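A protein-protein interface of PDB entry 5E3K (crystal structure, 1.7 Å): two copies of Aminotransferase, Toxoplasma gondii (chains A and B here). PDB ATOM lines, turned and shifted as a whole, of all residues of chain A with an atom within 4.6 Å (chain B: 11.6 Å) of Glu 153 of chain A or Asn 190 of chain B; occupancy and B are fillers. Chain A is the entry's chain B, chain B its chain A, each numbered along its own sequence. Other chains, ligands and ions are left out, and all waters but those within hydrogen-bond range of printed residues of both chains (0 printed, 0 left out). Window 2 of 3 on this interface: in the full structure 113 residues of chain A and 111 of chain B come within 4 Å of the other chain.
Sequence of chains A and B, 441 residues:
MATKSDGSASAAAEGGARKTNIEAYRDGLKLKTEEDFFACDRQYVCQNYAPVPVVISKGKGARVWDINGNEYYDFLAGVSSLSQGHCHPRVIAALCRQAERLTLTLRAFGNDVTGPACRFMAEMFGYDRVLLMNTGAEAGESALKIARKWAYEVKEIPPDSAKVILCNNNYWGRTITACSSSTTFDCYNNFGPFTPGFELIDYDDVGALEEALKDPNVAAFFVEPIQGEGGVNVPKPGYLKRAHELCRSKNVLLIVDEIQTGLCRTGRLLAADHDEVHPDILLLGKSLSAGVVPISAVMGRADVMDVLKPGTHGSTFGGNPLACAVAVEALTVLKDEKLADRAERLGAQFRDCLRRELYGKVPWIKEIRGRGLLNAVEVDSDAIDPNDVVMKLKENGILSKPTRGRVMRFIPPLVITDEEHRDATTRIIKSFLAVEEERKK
OG of Ser 180 of chain B lies within hydrogen-bond range of O of Ile 176 of chain B, 2.7 Å away.
The side-chain amino group of Lys 149 of chain A is in salt-bridge range of the side-chain carboxylate of Glu 153 of chain A (2.8 Å).
O of Val 307 of chain A lies within hydrogen-bond range of NZ of Lys 149 of chain A, 2.9 Å away.
No position is printed for both chains.
Of the 10 printed residues of chain A, 4 touch a printed residue of chain B.
Printed residues of chain A that touch a printed residue of chain B: Arg 148, Lys 149, Tyr 152 and Glu 153.
Among the printed residues, no Asp or Glu carboxylate lies within 4 Å of a Lys or Arg side-chain nitrogen of the other chain.
The backbone NH (N) of Lys 149 of chain A sits close to the backbone carbonyl oxygen (O) of Asn 190 of chain B, at 3.4 Å.
The side-chain amide nitrogen (ND2) of Asn 190 of chain B is in hydrogen-bond range of the side-chain carboxylate (OE2) of Glu 153 of chain A (3.2 Å).
The backbone carbonyl oxygen of Phe 191 of chain B lies within hydrogen-bond range of the guanidinium group of Arg 148 of chain A, 2.9 Å away.
The backbone carbonyl oxygen (O) of Gly 192 of chain B lies within hydrogen-bond range of the side-chain hydroxyl (OH) of Tyr 152 of chain A (2.7 Å).
O of Pro 193 of chain B lies within hydrogen-bond range of NH1 of Arg 148 of chain A (2.8 Å).
Arg 148 of chain A touches Ile 176 of chain B.
Asn 190 of chain B touches Arg 148 of chain A (O to C, 3.8 Å).
Arg 148 of chain A touches Gly 192 of chain B.
Asn 189 of chain B touches Lys 149 of chain A (O to CE, 3.98 Å).
CD of Lys 149 of chain A touches CE1 of Phe 191 of chain B, at 3.7 Å.
Tyr 152 of chain A touches Asn 190 of chain B (CD2 to O, 3.2 Å).
Tyr 152 of chain A touches Pro 193 of chain B (OH to CD, 3.8 Å).
Glu 153 of chain A touches just one residue of chain B: Asn 190.
Of chain A, only Arg 148 (3.8 Å), Lys 149 (3.3 Å), Tyr 152 (3.2 Å) and Glu 153 (3.2 Å) come within 4 Å of Asn 190 of chain B.
No residue of chain B comes within 4 Å of Ala 151 of chain A.
Of chain B, only Asn 190, Gly 192 and Pro 193 come within 4 Å of Tyr 152 of chain A.
No residue of chain B comes within 4 Å of Val 154 of chain A.
No residue of chain B comes within 4 Å of Glu 156 of chain A.
Printed residues of chain A within 4 Å of Ile 176 of chain B: Arg 148 (3.7 Å).
Printed residues of chain A within 4 Å of Pro 193 of chain B: Arg 148 (2.8 Å) and Tyr 152 (3.8 Å).
Of the printed residues of chain A, Asn 189 of chain B touches Lys 149 (3.98 Å).
Of the printed residues of chain B, Lys 149 of chain A touches Asn 189, Asn 190 and Phe 191.
Ser 180 of chain B touches none of the printed residues of chain A.
Phe 194 of chain B touches none of the printed residues of chain A.
The nearest printed residue of chain A that does not touch Asn 189 of chain B is Glu 153 of chain A (4.8 Å).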
ATOM      1  N   ARG A 148      32.160 -21.506  -9.682  1.00  0.00           N
ATOM      2  CA  ARG A 148      31.065 -20.528  -9.580  1.00  0.00           C
ATOM      3  C   ARG A 148      31.374 -19.512  -8.516  1.00  0.00           C
ATOM      4  O   ARG A 148      31.229 -18.297  -8.771  1.00  0.00           O
ATOM      5  CB  ARG A 148      29.704 -21.232  -9.295  1.00  0.00           C
ATOM      6  CG  ARG A 148      29.217 -22.089 -10.437  1.00  0.00           C
ATOM      7  CD  ARG A 148      28.039 -22.967  -9.989  1.00  0.00           C
ATOM      8  NE  ARG A 148      27.228 -23.390 -11.104  1.00  0.00           N
ATOM      9  CZ  ARG A 148      25.956 -23.831 -11.017  1.00  0.00           C
ATOM     10  NH1 ARG A 148      25.350 -23.969  -9.832  1.00  0.00           N
ATOM     11  NH2 ARG A 148      25.306 -24.151 -12.130  1.00  0.00           N
ATOM     12  N   LYS A 149      31.784 -19.951  -7.309  1.00  0.00           N
ATOM     13  CA  LYS A 149      32.017 -19.006  -6.205  1.00  0.00           C
ATOM     14  C   LYS A 149      33.156 -18.032  -6.566  1.00  0.00           C
ATOM     15  O   LYS A 149      33.107 -16.825  -6.221  1.00  0.00           O
ATOM     16  CB  LYS A 149      32.266 -19.742  -4.898  1.00  0.00           C
ATOM     17  CG  LYS A 149      32.330 -18.916  -3.641  1.00  0.00           C
ATOM     18  CD  LYS A 149      32.162 -19.745  -2.382  1.00  0.00           C
ATOM     19  CE  LYS A 149      31.827 -18.956  -1.131  1.00  0.00           C
ATOM     20  NZ  LYS A 149      32.979 -18.134  -0.691  1.00  0.00           N
ATOM     21  N   TRP A 150      34.162 -18.557  -7.248  1.00  0.00           N
ATOM     22  CA  TRP A 150      35.286 -17.722  -7.731  1.00  0.00           C
ATOM     23  C   TRP A 150      34.822 -16.690  -8.760  1.00  0.00           C
ATOM     24  O   TRP A 150      35.179 -15.512  -8.689  1.00  0.00           O
ATOM     25  CB  TRP A 150      36.370 -18.627  -8.325  1.00  0.00           C
ATOM     26  CG  TRP A 150      37.475 -17.876  -8.996  1.00  0.00           C
ATOM     27  CD1 TRP A 150      38.588 -17.343  -8.414  1.00  0.00           C
ATOM     28  CD2 TRP A 150      37.561 -17.576 -10.376  1.00  0.00           C
ATOM     29  NE1 TRP A 150      39.338 -16.696  -9.361  1.00  0.00           N
ATOM     30  CE2 TRP A 150      38.760 -16.918 -10.590  1.00  0.00           C
ATOM     31  CE3 TRP A 150      36.758 -17.897 -11.484  1.00  0.00           C
ATOM     32  CZ2 TRP A 150      39.150 -16.488 -11.858  1.00  0.00           C
ATOM     33  CZ3 TRP A 150      37.158 -17.479 -12.748  1.00  0.00           C
ATOM     34  CH2 TRP A 150      38.338 -16.791 -12.925  1.00  0.00           C
ATOM     35  N   ALA A 151      33.971 -17.124  -9.695  1.00  0.00           N
ATOM     36  CA  ALA A 151      33.420 -16.202 -10.661  1.00  0.00           C
ATOM     37  C   ALA A 151      32.632 -15.067 -10.004  1.00  0.00           C
ATOM     38  O   ALA A 151      32.747 -13.903 -10.430  1.00  0.00           O
ATOM     39  CB  ALA A 151      32.570 -16.949 -11.711  1.00  0.00           C
ATOM     40  N   TYR A 152      31.806 -15.406  -9.022  1.00  0.00           N
ATOM     41  CA  TYR A 152      31.016 -14.368  -8.327  1.00  0.00           C
ATOM     42  C   TYR A 152      31.912 -13.411  -7.561  1.00  0.00           C
ATOM     43  O   TYR A 152      31.649 -12.218  -7.575  1.00  0.00           O
ATOM     44  CB  TYR A 152      29.946 -14.967  -7.392  1.00  0.00           C
ATOM     45  CG  TYR A 152      28.920 -15.763  -8.174  1.00  0.00           C
ATOM     46  CD1 TYR A 152      28.249 -15.190  -9.287  1.00  0.00           C
ATOM     47  CD2 TYR A 152      28.618 -17.043  -7.823  1.00  0.00           C
ATOM     48  CE1 TYR A 152      27.346 -15.935 -10.046  1.00  0.00           C
ATOM     49  CE2 TYR A 152      27.714 -17.799  -8.542  1.00  0.00           C
ATOM     50  CZ  TYR A 152      27.097 -17.248  -9.668  1.00  0.00           C
ATOM     51  OH  TYR A 152      26.182 -17.984 -10.386  1.00  0.00           O
ATOM     52  N   GLU A 153      32.916 -13.944  -6.865  1.00  0.00           N
ATOM     53  CA  GLU A 153      33.715 -13.173  -5.904  1.00  0.00           C
ATOM     54  C   GLU A 153      34.913 -12.459  -6.577  1.00  0.00           C
ATOM     55  O   GLU A 153      35.228 -11.300  -6.224  1.00  0.00           O
ATOM     56  CB  GLU A 153      34.117 -14.055  -4.718  1.00  0.00           C
ATOM     57  CG  GLU A 153      32.901 -14.563  -3.945  1.00  0.00           C
ATOM     58  CD  GLU A 153      33.233 -15.448  -2.756  1.00  0.00           C
ATOM     59  OE1 GLU A 153      34.409 -15.703  -2.487  1.00  0.00           O
ATOM     60  OE2 GLU A 153      32.282 -15.838  -2.068  1.00  0.00           O
ATOM     61  N   VAL A 154      35.527 -13.112  -7.567  1.00  0.00           N
ATOM     62  CA  VAL A 154      36.770 -12.598  -8.178  1.00  0.00           C
ATOM     63  C   VAL A 154      36.492 -11.863  -9.490  1.00  0.00           C
ATOM     64  O   VAL A 154      36.919 -10.725  -9.659  1.00  0.00           O
ATOM     65  CB  VAL A 154      37.894 -13.649  -8.287  1.00  0.00           C
ATOM     66  CG1 VAL A 154      39.140 -13.021  -8.959  1.00  0.00           C
ATOM     67  CG2 VAL A 154      38.274 -14.129  -6.903  1.00  0.00           C
ATOM     68  N   LYS A 155      35.781 -12.502 -10.414  1.00  0.00           N
ATOM     69  CA  LYS A 155      35.331 -11.850 -11.654  1.00  0.00           C
ATOM     70  C   LYS A 155      34.113 -10.916 -11.466  1.00  0.00           C
ATOM     71  O   LYS A 155      33.803 -10.105 -12.361  1.00  0.00           O
ATOM     72  CB  LYS A 155      34.991 -12.903 -12.727  1.00  0.00           C
ATOM     73  CG  LYS A 155      36.155 -13.773 -13.165  1.00  0.00           C
ATOM     74  CD  LYS A 155      35.735 -14.901 -14.103  1.00  0.00           C
ATOM     75  CE  LYS A 155      34.920 -14.492 -15.293  1.00  0.00           C
ATOM     76  NZ  LYS A 155      35.267 -15.326 -16.479  1.00  0.00           N
ATOM     77  N   GLU A 156      33.407 -11.047 -10.335  1.00  0.00           N
ATOM     78  CA  GLU A 156      32.250 -10.169 -10.005  1.00  0.00           C
ATOM     79  C   GLU A 156      31.141 -10.195 -11.061  1.00  0.00           C
ATOM     80  O   GLU A 156      30.464  -9.193 -11.310  1.00  0.00           O
ATOM     81  CB  GLU A 156      32.706  -8.736  -9.757  1.00  0.00           C
ATOM     82  CG  GLU A 156      33.645  -8.591  -8.589  1.00  0.00           C
ATOM     83  CD  GLU A 156      34.021  -7.149  -8.352  1.00  0.00           C
ATOM     84  OE1 GLU A 156      33.232  -6.246  -8.702  1.00  0.00           O
ATOM     85  OE2 GLU A 156      35.127  -6.906  -7.862  1.00  0.00           O
ATOM     86  N   VAL A 307      38.603 -19.679  -2.178  1.00  0.00           N
ATOM     87  CA  VAL A 307      37.203 -19.207  -2.073  1.00  0.00           C
ATOM     88  C   VAL A 307      36.347 -20.169  -1.231  1.00  0.00           C
ATOM     89  O   VAL A 307      35.307 -19.794  -0.701  1.00  0.00           O
ATOM     90  CB  VAL A 307      36.538 -18.956  -3.445  1.00  0.00           C
ATOM     91  CG1 VAL A 307      37.302 -17.935  -4.229  1.00  0.00           C
ATOM     92  CG2 VAL A 307      36.232 -20.231  -4.200  1.00  0.00           C
ATOM     93  N   GLN B  47      41.134 -24.944   2.334  1.00  0.00           N
ATOM     94  CA  GLN B  47      40.834 -24.406   3.670  1.00  0.00           C
ATOM     95  C   GLN B  47      39.323 -24.268   4.006  1.00  0.00           C
ATOM     96  O   GLN B  47      38.879 -23.268   4.595  1.00  0.00           O
ATOM     97  CB  GLN B  47      41.510 -23.048   3.846  1.00  0.00           C
ATOM     98  CG  GLN B  47      40.994 -21.976   2.885  1.00  0.00           C
ATOM     99  CD  GLN B  47      41.152 -20.525   3.348  1.00  0.00           C
ATOM    100  OE1 GLN B  47      41.668 -20.275   4.408  1.00  0.00           O
ATOM    101  NE2 GLN B  47      40.704 -19.568   2.541  1.00  0.00           N
ATOM    102  N   ARG B 174      26.627 -31.911   0.195  1.00  0.00           N
ATOM    103  CA  ARG B 174      27.307 -30.725  -0.349  1.00  0.00           C
ATOM    104  C   ARG B 174      27.347 -30.668  -1.864  1.00  0.00           C
ATOM    105  O   ARG B 174      27.998 -29.776  -2.452  1.00  0.00           O
ATOM    106  CB  ARG B 174      28.717 -30.640   0.240  1.00  0.00           C
ATOM    107  CG  ARG B 174      28.740 -30.485   1.742  1.00  0.00           C
ATOM    108  CD  ARG B 174      28.398 -29.044   2.149  1.00  0.00           C
ATOM    109  NE  ARG B 174      28.662 -28.832   3.541  1.00  0.00           N
ATOM    110  CZ  ARG B 174      28.899 -27.649   4.082  1.00  0.00           C
ATOM    111  NH1 ARG B 174      28.818 -26.556   3.345  1.00  0.00           N
ATOM    112  NH2 ARG B 174      29.235 -27.588   5.350  1.00  0.00           N
ATOM    113  N   THR B 175      26.634 -31.568  -2.539  1.00  0.00           N
ATOM    114  CA  THR B 175      26.445 -31.400  -3.982  1.00  0.00           C
ATOM    115  C   THR B 175      25.658 -30.120  -4.280  1.00  0.00           C
ATOM    116  O   THR B 175      24.977 -29.549  -3.381  1.00  0.00           O
ATOM    117  CB  THR B 175      25.694 -32.589  -4.578  1.00  0.00           C
ATOM    118  OG1 THR B 175      24.403 -32.602  -3.997  1.00  0.00           O
ATOM    119  CG2 THR B 175      26.428 -33.878  -4.348  1.00  0.00           C
ATOM    120  N   ILE B 176      25.707 -29.672  -5.532  1.00  0.00           N
ATOM    121  CA  ILE B 176      24.967 -28.453  -5.928  1.00  0.00           C
ATOM    122  C   ILE B 176      23.459 -28.628  -5.668  1.00  0.00           C
ATOM    123  O   ILE B 176      22.799 -27.727  -5.141  1.00  0.00           O
ATOM    124  CB  ILE B 176      25.305 -27.963  -7.361  1.00  0.00           C
ATOM    125  CG1 ILE B 176      26.773 -27.376  -7.380  1.00  0.00           C
ATOM    126  CG2 ILE B 176      24.270 -26.974  -7.898  1.00  0.00           C
ATOM    127  CD1 ILE B 176      27.417 -27.211  -8.738  1.00  0.00           C
ATOM    128  N   THR B 177      22.927 -29.809  -5.955  1.00  0.00           N
ATOM    129  CA  THR B 177      21.543 -30.018  -5.685  1.00  0.00           C
ATOM    130  C   THR B 177      21.230 -29.977  -4.189  1.00  0.00           C
ATOM    131  O   THR B 177      20.160 -29.483  -3.813  1.00  0.00           O
ATOM    132  CB  THR B 177      21.018 -31.289  -6.413  1.00  0.00           C
ATOM    133  OG1 THR B 177      21.182 -31.087  -7.819  1.00  0.00           O
ATOM    134  CG2 THR B 177      19.592 -31.558  -6.091  1.00  0.00           C
ATOM    135  N   CYS B 179      22.950 -28.126  -2.077  1.00  0.00           N
ATOM    136  CA  CYS B 179      23.059 -26.689  -1.744  1.00  0.00           C
ATOM    137  C   CYS B 179      21.774 -25.955  -2.167  1.00  0.00           C
ATOM    138  O   CYS B 179      21.310 -25.075  -1.448  1.00  0.00           O
ATOM    139  CB  CYS B 179      24.242 -26.071  -2.414  1.00  0.00           C
ATOM    140  SG  CYS B 179      25.845 -26.729  -1.903  1.00  0.00           S
ATOM    141  N   SER B 180      21.200 -26.383  -3.285  1.00  0.00           N
ATOM    142  CA  SER B 180      19.980 -25.838  -3.846  1.00  0.00           C
ATOM    143  C   SER B 180      18.744 -26.077  -2.983  1.00  0.00           C
ATOM    144  O   SER B 180      17.733 -25.405  -3.181  1.00  0.00           O
ATOM    145  CB  SER B 180      19.712 -26.482  -5.193  1.00  0.00           C
ATOM    146  OG  SER B 180      20.775 -26.303  -6.098  1.00  0.00           O
ATOM    147  N   SER B 182      18.994 -26.248   0.586  1.00  0.00           N
ATOM    148  CA  SER B 182      19.461 -25.877   1.917  1.00  0.00           C
ATOM    149  C   SER B 182      18.887 -24.519   2.256  1.00  0.00           C
ATOM    150  O   SER B 182      18.685 -23.687   1.372  1.00  0.00           O
ATOM    151  CB  SER B 182      21.001 -25.710   1.970  1.00  0.00           C
ATOM    152  OG  SER B 182      21.501 -25.507   3.282  1.00  0.00           O
ATOM    153  N   THR B 183      18.711 -24.292   3.546  1.00  0.00           N
ATOM    154  CA  THR B 183      18.401 -22.955   4.070  1.00  0.00           C
ATOM    155  C   THR B 183      19.560 -22.390   4.874  1.00  0.00           C
ATOM    156  O   THR B 183      19.400 -21.342   5.529  1.00  0.00           O
ATOM    157  CB  THR B 183      17.120 -22.931   4.937  1.00  0.00           C
ATOM    158  OG1 THR B 183      17.294 -23.711   6.137  1.00  0.00           O
ATOM    159  CG2 THR B 183      15.960 -23.405   4.185  1.00  0.00           C
ATOM    160  N   THR B 184      20.733 -23.018   4.780  1.00  0.00           N
ATOM    161  CA  THR B 184      21.891 -22.545   5.521  1.00  0.00           C
ATOM    162  C   THR B 184      22.786 -21.671   4.629  1.00  0.00           C
ATOM    163  O   THR B 184      23.339 -22.117   3.658  1.00  0.00           O
ATOM    164  CB  THR B 184      22.692 -23.730   6.014  1.00  0.00           C
ATOM    165  OG1 THR B 184      21.848 -24.602   6.770  1.00  0.00           O
ATOM    166  CG2 THR B 184      23.880 -23.283   6.906  1.00  0.00           C
ATOM    167  N   PHE B 185      22.956 -20.392   4.981  1.00  0.00           N
ATOM    168  CA  PHE B 185      23.574 -19.432   4.081  1.00  0.00           C
ATOM    169  C   PHE B 185      24.907 -19.920   3.530  1.00  0.00           C
ATOM    170  O   PHE B 185      25.130 -19.892   2.343  1.00  0.00           O
ATOM    171  CB  PHE B 185      23.787 -18.095   4.812  1.00  0.00           C
ATOM    172  CG  PHE B 185      24.386 -17.012   3.944  1.00  0.00           C
ATOM    173  CD1 PHE B 185      23.610 -16.361   2.987  1.00  0.00           C
ATOM    174  CD2 PHE B 185      25.715 -16.649   4.084  1.00  0.00           C
ATOM    175  CE1 PHE B 185      24.150 -15.366   2.187  1.00  0.00           C
ATOM    176  CE2 PHE B 185      26.279 -15.649   3.296  1.00  0.00           C
ATOM    177  CZ  PHE B 185      25.498 -15.001   2.331  1.00  0.00           C
ATOM    178  N   ASP B 186      25.804 -20.392   4.396  1.00  0.00           N
ATOM    179  CA  ASP B 186      27.117 -20.781   3.899  1.00  0.00           C
ATOM    180  C   ASP B 186      27.090 -22.035   3.069  1.00  0.00           C
ATOM    181  O   ASP B 186      27.997 -22.252   2.296  1.00  0.00           O
ATOM    182  CB  ASP B 186      28.154 -20.938   5.023  1.00  0.00           C
ATOM    183  CG  ASP B 186      28.726 -19.585   5.498  1.00  0.00           C
ATOM    184  OD1 ASP B 186      28.841 -18.620   4.717  1.00  0.00           O
ATOM    185  OD2 ASP B 186      29.162 -19.555   6.659  1.00  0.00           O
ATOM    186  N   CYS B 187      26.052 -22.856   3.199  1.00  0.00           N
ATOM    187  CA  CYS B 187      25.912 -23.996   2.316  1.00  0.00           C
ATOM    188  C   CYS B 187      25.602 -23.597   0.883  1.00  0.00           C
ATOM    189  O   CYS B 187      26.133 -24.193  -0.040  1.00  0.00           O
ATOM    190  CB  CYS B 187      24.850 -24.966   2.792  1.00  0.00           C
ATOM    191  SG  CYS B 187      25.438 -25.916   4.171  1.00  0.00           S
ATOM    192  N   TYR B 188      24.736 -22.613   0.684  1.00  0.00           N
ATOM    193  CA  TYR B 188      24.305 -22.280  -0.681  1.00  0.00           C
ATOM    194  C   TYR B 188      24.939 -21.031  -1.266  1.00  0.00           C
ATOM    195  O   TYR B 188      24.919 -20.883  -2.497  1.00  0.00           O
ATOM    196  CB  TYR B 188      22.767 -22.153  -0.803  1.00  0.00           C
ATOM    197  CG  TYR B 188      22.120 -21.036  -0.008  1.00  0.00           C
ATOM    198  CD1 TYR B 188      22.200 -19.683  -0.420  1.00  0.00           C
ATOM    199  CD2 TYR B 188      21.419 -21.314   1.176  1.00  0.00           C
ATOM    200  CE1 TYR B 188      21.626 -18.680   0.358  1.00  0.00           C
ATOM    201  CE2 TYR B 188      20.851 -20.296   1.965  1.00  0.00           C
ATOM    202  CZ  TYR B 188      20.954 -18.992   1.537  1.00  0.00           C
ATOM    203  OH  TYR B 188      20.373 -17.923   2.250  1.00  0.00           O
ATOM    204  N   ASN B 189      25.406 -20.067  -0.451  1.00  0.00           N
ATOM    205  CA  ASN B 189      25.769 -18.781  -0.982  1.00  0.00           C
ATOM    206  C   ASN B 189      26.839 -18.901  -2.077  1.00  0.00           C
ATOM    207  O   ASN B 189      27.935 -19.440  -1.834  1.00  0.00           O
ATOM    208  CB  ASN B 189      26.325 -17.889   0.155  1.00  0.00           C
ATOM    209  CG  ASN B 189      26.758 -16.513  -0.289  1.00  0.00           C
ATOM    210  OD1 ASN B 189      26.000 -15.757  -0.883  1.00  0.00           O
ATOM    211  ND2 ASN B 189      27.997 -16.146   0.060  1.00  0.00           N
ATOM    212  N   ASN B 190      26.575 -18.222  -3.186  1.00  0.00           N
ATOM    213  CA  ASN B 190      27.490 -18.103  -4.326  1.00  0.00           C
ATOM    214  C   ASN B 190      27.792 -19.396  -5.033  1.00  0.00           C
ATOM    215  O   ASN B 190      28.786 -19.506  -5.765  1.00  0.00           O
ATOM    216  CB  ASN B 190      28.781 -17.337  -3.962  1.00  0.00           C
ATOM    217  CG  ASN B 190      28.576 -15.846  -3.937  1.00  0.00           C
ATOM    218  OD1 ASN B 190      27.600 -15.344  -4.461  1.00  0.00           O
ATOM    219  ND2 ASN B 190      29.473 -15.129  -3.306  1.00  0.00           N
ATOM    220  N   PHE B 191      26.918 -20.377  -4.866  1.00  0.00           N
ATOM    221  CA  PHE B 191      27.046 -21.628  -5.551  1.00  0.00           C
ATOM    222  C   PHE B 191      25.981 -21.880  -6.618  1.00  0.00           C
ATOM    223  O   PHE B 191      25.923 -22.984  -7.217  1.00  0.00           O
ATOM    224  CB  PHE B 191      27.071 -22.800  -4.547  1.00  0.00           C
ATOM    225  CG  PHE B 191      28.273 -22.857  -3.659  1.00  0.00           C
ATOM    226  CD1 PHE B 191      29.569 -22.834  -4.139  1.00  0.00           C
ATOM    227  CD2 PHE B 191      28.077 -23.038  -2.281  1.00  0.00           C
ATOM    228  CE1 PHE B 191      30.645 -22.942  -3.280  1.00  0.00           C
ATOM    229  CE2 PHE B 191      29.137 -23.079  -1.408  1.00  0.00           C
ATOM    230  CZ  PHE B 191      30.422 -23.064  -1.905  1.00  0.00           C
ATOM    231  N   GLY B 192      25.116 -20.910  -6.866  1.00  0.00           N
ATOM    232  CA  GLY B 192      24.044 -21.078  -7.898  1.00  0.00           C
ATOM    233  C   GLY B 192      24.517 -20.828  -9.318  1.00  0.00           C
ATOM    234  O   GLY B 192      25.690 -20.465  -9.543  1.00  0.00           O
ATOM    235  N   PRO B 193      23.640 -20.966 -10.319  1.00  0.00           N
ATOM    236  CA  PRO B 193      22.207 -21.117 -10.146  1.00  0.00           C
ATOM    237  C   PRO B 193      21.819 -22.538  -9.706  1.00  0.00           C
ATOM    238  O   PRO B 193      22.590 -23.511  -9.894  1.00  0.00           O
ATOM    239  CB  PRO B 193      21.658 -20.778 -11.534  1.00  0.00           C
ATOM    240  CG  PRO B 193      22.758 -21.167 -12.479  1.00  0.00           C
ATOM    241  CD  PRO B 193      24.014 -20.789 -11.742  1.00  0.00           C
ATOM    242  N   PHE B 194      20.645 -22.612  -9.103  1.00  0.00           N
ATOM    243  CA  PHE B 194      20.277 -23.734  -8.279  1.00  0.00           C
ATOM    244  C   PHE B 194      19.349 -24.679  -9.007  1.00  0.00           C
ATOM    245  O   PHE B 194      18.551 -24.266  -9.882  1.00  0.00           O
ATOM    246  CB  PHE B 194      19.678 -23.285  -6.938  1.00  0.00           C
ATOM    247  CG  PHE B 194      20.636 -22.437  -6.109  1.00  0.00           C
ATOM    248  CD1 PHE B 194      21.766 -23.020  -5.521  1.00  0.00           C
ATOM    249  CD2 PHE B 194      20.473 -21.068  -6.018  1.00  0.00           C
ATOM    250  CE1 PHE B 194      22.633 -22.222  -4.763  1.00  0.00           C
ATOM    251  CE2 PHE B 194      21.348 -20.282  -5.260  1.00  0.00           C
ATOM    252  CZ  PHE B 194      22.431 -20.845  -4.645  1.00  0.00           C
ATOM    253  N   THR B 195      19.414 -25.916  -8.590  1.00  0.00           N
ATOM    254  CA  THR B 195      18.473 -26.940  -9.069  1.00  0.00           C
ATOM    255  C   THR B 195      17.044 -26.533  -8.594  1.00  0.00           C
ATOM    256  O   THR B 195      16.843 -26.345  -7.401  1.00  0.00           O
ATOM    257  CB  THR B 195      18.835 -28.309  -8.504  1.00  0.00           C
ATOM    258  OG1 THR B 195      20.226 -28.621  -8.753  1.00  0.00           O
ATOM    259  CG2 THR B 195      17.986 -29.373  -9.134  1.00  0.00           C
